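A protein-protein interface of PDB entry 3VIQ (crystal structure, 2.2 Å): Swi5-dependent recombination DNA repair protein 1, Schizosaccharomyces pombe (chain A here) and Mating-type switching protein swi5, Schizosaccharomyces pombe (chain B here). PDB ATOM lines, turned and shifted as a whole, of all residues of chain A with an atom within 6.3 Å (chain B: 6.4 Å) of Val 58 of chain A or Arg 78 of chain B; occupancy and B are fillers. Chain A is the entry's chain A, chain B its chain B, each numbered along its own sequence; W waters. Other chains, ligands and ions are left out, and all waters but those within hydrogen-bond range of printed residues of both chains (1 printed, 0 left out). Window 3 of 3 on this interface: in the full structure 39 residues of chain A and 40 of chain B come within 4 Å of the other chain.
Of the printed residues of chain B, Ala 55 of chain A touches Phe 79. Val 58 of chain A touches just one residue of chain B: Arg 78. Of the printed residues of chain B, Leu 59 of chain A touches Val 64 (3.8 Å). Of the printed residues of chain A, Val 64 of chain B touches Leu 59. Printed residues of chain A within 4 Å of Arg 78 of chain B: Gln 54 (2.8 Å) and Val 58 (3.7 Å). Printed residues of chain A within 4 Å of Phe 79 of chain B: Gln 54 (3.7 Å) and Ala 55 (3.7 Å).
Phe 79 of chain B touches Gln 54 of chain A (CD1 to CD, 3.7 Å). Ala 55 of chain A touches Phe 79 of chain B (N to CE1, 3.7 Å). CG1 of Val 58 of chain A touches NH2 of Arg 78 of chain B (3.7 Å). CG2 of Val 64 of chain B touches CG of Leu 59 of chain A, at 3.8 Å.
Water W1 lies within hydrogen-bond range of O of Arg 78 of chain B (2.9 Å) and OE1 of Gln 54 of chain A (2.9 Å).
The guanidinium group of Arg 78 of chain B is in salt-bridge range of the side-chain carboxylate of Glu 68 of chain B (3.3 Å).
The backbone carbonyl oxygen of Arg 78 of chain B sits at hydrogen-bond distance from the side-chain amide nitrogen of Gln 54 of chain A.
Of the 11 printed residues of chain A, 4 touch a printed residue of chain B. Among the printed residues, 5 pairs touch across the chains.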
ATOM      1  N   GLN A  53     -16.580 -18.552   2.869  1.00  0.00           N
ATOM      2  CA  GLN A  53     -15.852 -17.744   3.878  1.00  0.00           C
ATOM      3  C   GLN A  53     -14.709 -16.883   3.300  1.00  0.00           C
ATOM      4  O   GLN A  53     -14.560 -15.678   3.618  1.00  0.00           O
ATOM      5  CB  GLN A  53     -15.302 -18.664   4.998  1.00  0.00           C
ATOM      6  CG  GLN A  53     -16.412 -19.350   5.821  1.00  0.00           C
ATOM      7  CD  GLN A  53     -15.926 -20.359   6.856  1.00  0.00           C
ATOM      8  OE1 GLN A  53     -14.752 -20.694   6.915  1.00  0.00           O
ATOM      9  NE2 GLN A  53     -16.854 -20.865   7.664  1.00  0.00           N
ATOM     10  N   GLN A  54     -13.880 -17.518   2.498  1.00  0.00           N
ATOM     11  CA  GLN A  54     -12.798 -16.846   1.792  1.00  0.00           C
ATOM     12  C   GLN A  54     -13.365 -15.746   0.882  1.00  0.00           C
ATOM     13  O   GLN A  54     -12.895 -14.591   0.929  1.00  0.00           O
ATOM     14  CB  GLN A  54     -12.058 -17.903   0.971  1.00  0.00           C
ATOM     15  CG  GLN A  54     -10.700 -17.557   0.472  1.00  0.00           C
ATOM     16  CD  GLN A  54     -10.047 -18.726  -0.299  1.00  0.00           C
ATOM     17  OE1 GLN A  54     -10.410 -19.899  -0.124  1.00  0.00           O
ATOM     18  NE2 GLN A  54      -9.095 -18.394  -1.164  1.00  0.00           N
ATOM     19  N   ALA A  55     -14.384 -16.087   0.069  1.00  0.00           N
ATOM     20  CA  ALA A  55     -15.018 -15.098  -0.819  1.00  0.00           C
ATOM     21  C   ALA A  55     -15.719 -13.987  -0.022  1.00  0.00           C
ATOM     22  O   ALA A  55     -15.662 -12.811  -0.416  1.00  0.00           O
ATOM     23  CB  ALA A  55     -16.007 -15.767  -1.782  1.00  0.00           C
ATOM     24  N   ALA A  56     -16.384 -14.345   1.079  1.00  0.00           N
ATOM     25  CA  ALA A  56     -16.994 -13.332   1.959  1.00  0.00           C
ATOM     26  C   ALA A  56     -15.965 -12.316   2.479  1.00  0.00           C
ATOM     27  O   ALA A  56     -16.245 -11.128   2.519  1.00  0.00           O
ATOM     28  CB  ALA A  56     -17.745 -13.982   3.139  1.00  0.00           C
ATOM     29  N   GLU A  57     -14.791 -12.785   2.883  1.00  0.00           N
ATOM     30  CA  GLU A  57     -13.708 -11.903   3.352  1.00  0.00           C
ATOM     31  C   GLU A  57     -13.160 -10.977   2.252  1.00  0.00           C
ATOM     32  O   GLU A  57     -12.817  -9.809   2.518  1.00  0.00           O
ATOM     33  CB  GLU A  57     -12.565 -12.731   3.940  1.00  0.00           C
ATOM     34  CG  GLU A  57     -12.830 -13.193   5.365  1.00  0.00           C
ATOM     35  CD  GLU A  57     -11.702 -14.033   5.919  1.00  0.00           C
ATOM     36  OE1 GLU A  57     -10.559 -13.860   5.465  1.00  0.00           O
ATOM     37  OE2 GLU A  57     -11.956 -14.880   6.801  1.00  0.00           O
ATOM     38  N   VAL A  58     -13.080 -11.488   1.023  1.00  0.00           N
ATOM     39  CA  VAL A  58     -12.652 -10.660  -0.110  1.00  0.00           C
ATOM     40  C   VAL A  58     -13.695  -9.569  -0.423  1.00  0.00           C
ATOM     41  O   VAL A  58     -13.318  -8.434  -0.684  1.00  0.00           O
ATOM     42  CB  VAL A  58     -12.410 -11.493  -1.391  1.00  0.00           C
ATOM     43  CG1 VAL A  58     -11.951 -10.592  -2.525  1.00  0.00           C
ATOM     44  CG2 VAL A  58     -11.362 -12.601  -1.140  1.00  0.00           C
ATOM     45  N   LEU A  59     -14.990  -9.914  -0.406  1.00  0.00           N
ATOM     46  CA  LEU A  59     -16.041  -8.942  -0.763  1.00  0.00           C
ATOM     47  C   LEU A  59     -16.341  -7.934   0.358  1.00  0.00           C
ATOM     48  O   LEU A  59     -16.508  -6.718   0.100  1.00  0.00           O
ATOM     49  CB  LEU A  59     -17.336  -9.640  -1.152  1.00  0.00           C
ATOM     50  CG  LEU A  59     -17.280 -10.402  -2.461  1.00  0.00           C
ATOM     51  CD1 LEU A  59     -18.304 -11.559  -2.429  1.00  0.00           C
ATOM     52  CD2 LEU A  59     -17.497  -9.470  -3.628  1.00  0.00           C
ATOM     53  N   PHE A  60     -16.391  -8.453   1.588  1.00  0.00           N
ATOM     54  CA  PHE A  60     -16.737  -7.657   2.782  1.00  0.00           C
ATOM     55  C   PHE A  60     -15.831  -6.461   2.948  1.00  0.00           C
ATOM     56  O   PHE A  60     -16.323  -5.360   3.137  1.00  0.00           O
ATOM     57  CB  PHE A  60     -16.695  -8.503   4.074  1.00  0.00           C
ATOM     58  CG  PHE A  60     -16.776  -7.691   5.356  1.00  0.00           C
ATOM     59  CD1 PHE A  60     -17.947  -7.028   5.696  1.00  0.00           C
ATOM     60  CD2 PHE A  60     -15.675  -7.613   6.224  1.00  0.00           C
ATOM     61  CE1 PHE A  60     -18.032  -6.278   6.889  1.00  0.00           C
ATOM     62  CE2 PHE A  60     -15.722  -6.862   7.415  1.00  0.00           C
ATOM     63  CZ  PHE A  60     -16.892  -6.180   7.754  1.00  0.00           C
ATOM     64  N   LYS A  61     -14.520  -6.674   2.888  1.00  0.00           N
ATOM     65  CA  LYS A  61     -13.574  -5.648   3.364  1.00  0.00           C
ATOM     66  C   LYS A  61     -13.700  -4.288   2.641  1.00  0.00           C
ATOM     67  O   LYS A  61     -13.856  -3.247   3.316  1.00  0.00           O
ATOM     68  CB  LYS A  61     -12.113  -6.146   3.367  1.00  0.00           C
ATOM     69  CG  LYS A  61     -11.206  -5.279   4.251  1.00  0.00           C
ATOM     70  CD  LYS A  61      -9.748  -5.714   4.242  1.00  0.00           C
ATOM     71  CE  LYS A  61      -9.019  -5.242   2.993  1.00  0.00           C
ATOM     72  NZ  LYS A  61      -7.735  -4.593   3.356  1.00  0.00           N
ATOM     73  N   PRO A  62     -13.639  -4.288   1.286  1.00  0.00           N
ATOM     74  CA  PRO A  62     -13.871  -3.015   0.588  1.00  0.00           C
ATOM     75  C   PRO A  62     -15.349  -2.551   0.641  1.00  0.00           C
ATOM     76  O   PRO A  62     -15.604  -1.347   0.655  1.00  0.00           O
ATOM     77  CB  PRO A  62     -13.377  -3.281  -0.844  1.00  0.00           C
ATOM     78  CG  PRO A  62     -13.481  -4.794  -1.022  1.00  0.00           C
ATOM     79  CD  PRO A  62     -13.288  -5.392   0.357  1.00  0.00           C
ATOM     80  N   MET A  63     -16.304  -3.466   0.714  1.00  0.00           N
ATOM     81  CA  MET A  63     -17.706  -3.061   0.971  1.00  0.00           C
ATOM     82  C   MET A  63     -17.864  -2.269   2.289  1.00  0.00           C
ATOM     83  O   MET A  63     -18.482  -1.208   2.291  1.00  0.00           O
ATOM     84  CB  MET A  63     -18.654  -4.277   0.957  1.00  0.00           C
ATOM     85  CG  MET A  63     -20.114  -3.913   1.129  1.00  0.00           C
ATOM     86  SD  MET A  63     -21.255  -5.321   0.986  1.00  0.00           S
ATOM     87  CE  MET A  63     -22.846  -4.454   1.040  1.00  0.00           C
ATOM     88  N   VAL B  64     -17.243 -11.752  -6.738  1.00  0.00           N
ATOM     89  CA  VAL B  64     -15.815 -11.489  -6.884  1.00  0.00           C
ATOM     90  C   VAL B  64     -15.468 -11.488  -8.369  1.00  0.00           C
ATOM     91  O   VAL B  64     -14.689 -10.653  -8.816  1.00  0.00           O
ATOM     92  CB  VAL B  64     -14.918 -12.527  -6.185  1.00  0.00           C
ATOM     93  CG1 VAL B  64     -13.424 -12.166  -6.393  1.00  0.00           C
ATOM     94  CG2 VAL B  64     -15.265 -12.650  -4.699  1.00  0.00           C
ATOM     95  N   GLU B  68     -13.658  -8.585 -10.918  1.00  0.00           N
ATOM     96  CA  GLU B  68     -12.458  -8.921 -11.721  1.00  0.00           C
ATOM     97  C   GLU B  68     -12.707  -9.094 -13.223  1.00  0.00           C
ATOM     98  O   GLU B  68     -11.788  -9.425 -13.945  1.00  0.00           O
ATOM     99  CB  GLU B  68     -11.787 -10.180 -11.180  1.00  0.00           C
ATOM    100  CG  GLU B  68     -11.496 -10.094  -9.708  1.00  0.00           C
ATOM    101  CD  GLU B  68     -10.196 -10.734  -9.329  1.00  0.00           C
ATOM    102  OE1 GLU B  68      -9.892 -11.836  -9.830  1.00  0.00           O
ATOM    103  OE2 GLU B  68      -9.475 -10.137  -8.514  1.00  0.00           O
ATOM    104  N   GLU B  74     -12.976 -19.122 -13.770  1.00  0.00           N
ATOM    105  CA  GLU B  74     -11.575 -18.733 -13.690  1.00  0.00           C
ATOM    106  C   GLU B  74     -11.134 -18.517 -12.228  1.00  0.00           C
ATOM    107  O   GLU B  74      -9.934 -18.568 -11.918  1.00  0.00           O
ATOM    108  CB  GLU B  74     -11.312 -17.510 -14.554  1.00  0.00           C
ATOM    109  CG  GLU B  74     -11.691 -17.728 -16.036  1.00  0.00           C
ATOM    110  CD  GLU B  74     -11.580 -16.464 -16.880  1.00  0.00           C
ATOM    111  OE1 GLU B  74     -10.587 -15.711 -16.717  1.00  0.00           O
ATOM    112  OE2 GLU B  74     -12.483 -16.232 -17.724  1.00  0.00           O
ATOM    113  N   LEU B  75     -12.085 -18.355 -11.309  1.00  0.00           N
ATOM    114  CA  LEU B  75     -11.724 -18.141  -9.897  1.00  0.00           C
ATOM    115  C   LEU B  75     -11.830 -19.386  -9.020  1.00  0.00           C
ATOM    116  O   LEU B  75     -11.430 -19.371  -7.820  1.00  0.00           O
ATOM    117  CB  LEU B  75     -12.563 -17.015  -9.288  1.00  0.00           C
ATOM    118  CG  LEU B  75     -12.461 -15.652  -9.944  1.00  0.00           C
ATOM    119  CD1 LEU B  75     -13.283 -15.655 -11.225  1.00  0.00           C
ATOM    120  CD2 LEU B  75     -12.969 -14.605  -8.981  1.00  0.00           C
ATOM    121  N   PHE B  76     -12.329 -20.475  -9.604  1.00  0.00           N
ATOM    122  CA  PHE B  76     -12.563 -21.718  -8.826  1.00  0.00           C
ATOM    123  C   PHE B  76     -11.301 -22.229  -8.137  1.00  0.00           C
ATOM    124  O   PHE B  76     -11.355 -22.659  -6.977  1.00  0.00           O
ATOM    125  CB  PHE B  76     -13.195 -22.784  -9.719  1.00  0.00           C
ATOM    126  CG  PHE B  76     -14.699 -22.603  -9.950  1.00  0.00           C
ATOM    127  CD1 PHE B  76     -15.397 -21.475  -9.467  1.00  0.00           C
ATOM    128  CD2 PHE B  76     -15.423 -23.584 -10.633  1.00  0.00           C
ATOM    129  CE1 PHE B  76     -16.797 -21.331  -9.679  1.00  0.00           C
ATOM    130  CE2 PHE B  76     -16.798 -23.456 -10.847  1.00  0.00           C
ATOM    131  CZ  PHE B  76     -17.494 -22.322 -10.369  1.00  0.00           C
ATOM    132  N   ASP B  77     -10.154 -22.150  -8.807  1.00  0.00           N
ATOM    133  CA  ASP B  77      -8.920 -22.649  -8.184  1.00  0.00           C
ATOM    134  C   ASP B  77      -8.506 -21.862  -6.957  1.00  0.00           C
ATOM    135  O   ASP B  77      -8.105 -22.441  -5.952  1.00  0.00           O
ATOM    136  CB  ASP B  77      -7.766 -22.674  -9.171  1.00  0.00           C
ATOM    137  CG  ASP B  77      -7.871 -23.813 -10.127  1.00  0.00           C
ATOM    138  OD1 ASP B  77      -8.312 -24.913  -9.714  1.00  0.00           O
ATOM    139  OD2 ASP B  77      -7.523 -23.612 -11.300  1.00  0.00           O
ATOM    140  N   ARG B  78      -8.582 -20.548  -7.071  1.00  0.00           N
ATOM    141  CA  ARG B  78      -8.287 -19.630  -5.976  1.00  0.00           C
ATOM    142  C   ARG B  78      -9.133 -19.933  -4.736  1.00  0.00           C
ATOM    143  O   ARG B  78      -8.667 -19.782  -3.599  1.00  0.00           O
ATOM    144  CB  ARG B  78      -8.571 -18.207  -6.447  1.00  0.00           C
ATOM    145  CG  ARG B  78      -8.545 -17.143  -5.373  1.00  0.00           C
ATOM    146  CD  ARG B  78      -8.359 -15.769  -6.000  1.00  0.00           C
ATOM    147  NE  ARG B  78      -8.953 -14.731  -5.168  1.00  0.00           N
ATOM    148  CZ  ARG B  78      -9.408 -13.568  -5.619  1.00  0.00           C
ATOM    149  NH1 ARG B  78      -9.344 -13.255  -6.916  1.00  0.00           N
ATOM    150  NH2 ARG B  78      -9.943 -12.717  -4.757  1.00  0.00           N
ATOM    151  N   PHE B  79     -10.366 -20.369  -4.968  1.00  0.00           N
ATOM    152  CA  PHE B  79     -11.274 -20.718  -3.876  1.00  0.00           C
ATOM    153  C   PHE B  79     -11.333 -22.189  -3.488  1.00  0.00           C
ATOM    154  O   PHE B  79     -12.078 -22.538  -2.592  1.00  0.00           O
ATOM    155  CB  PHE B  79     -12.667 -20.140  -4.156  1.00  0.00           C
ATOM    156  CG  PHE B  79     -12.665 -18.644  -4.176  1.00  0.00           C
ATOM    157  CD1 PHE B  79     -12.430 -17.933  -3.007  1.00  0.00           C
ATOM    158  CD2 PHE B  79     -12.814 -17.934  -5.375  1.00  0.00           C
ATOM    159  CE1 PHE B  79     -12.381 -16.537  -3.019  1.00  0.00           C
ATOM    160  CE2 PHE B  79     -12.751 -16.553  -5.388  1.00  0.00           C
ATOM    161  CZ  PHE B  79     -12.541 -15.854  -4.198  1.00  0.00           C
ATOM    162  N   GLY B  80     -10.540 -23.045  -4.140  1.00  0.00           N
ATOM    163  CA  GLY B  80     -10.414 -24.443  -3.715  1.00  0.00           C
ATOM    164  C   GLY B  80     -11.510 -25.363  -4.212  1.00  0.00           C
ATOM    165  O   GLY B  80     -11.680 -26.459  -3.686  1.00  0.00           O
ATOM    166  N   VAL B  81     -12.221 -24.942  -5.249  1.00  0.00           N
ATOM    167  CA  VAL B  81     -13.312 -25.717  -5.806  1.00  0.00           C
ATOM    168  C   VAL B  81     -13.140 -25.983  -7.301  1.00  0.00           C
ATOM    169  O   VAL B  81     -12.257 -25.438  -7.951  1.00  0.00           O
ATOM    170  CB  VAL B  81     -14.671 -25.043  -5.572  1.00  0.00           C
ATOM    171  CG1 VAL B  81     -15.015 -25.083  -4.100  1.00  0.00           C
ATOM    172  CG2 VAL B  81     -14.668 -23.608  -6.056  1.00  0.00           C
HETATM  173  O   HOH W   1      -8.519 -21.718  -1.425  1.00  0.00           O
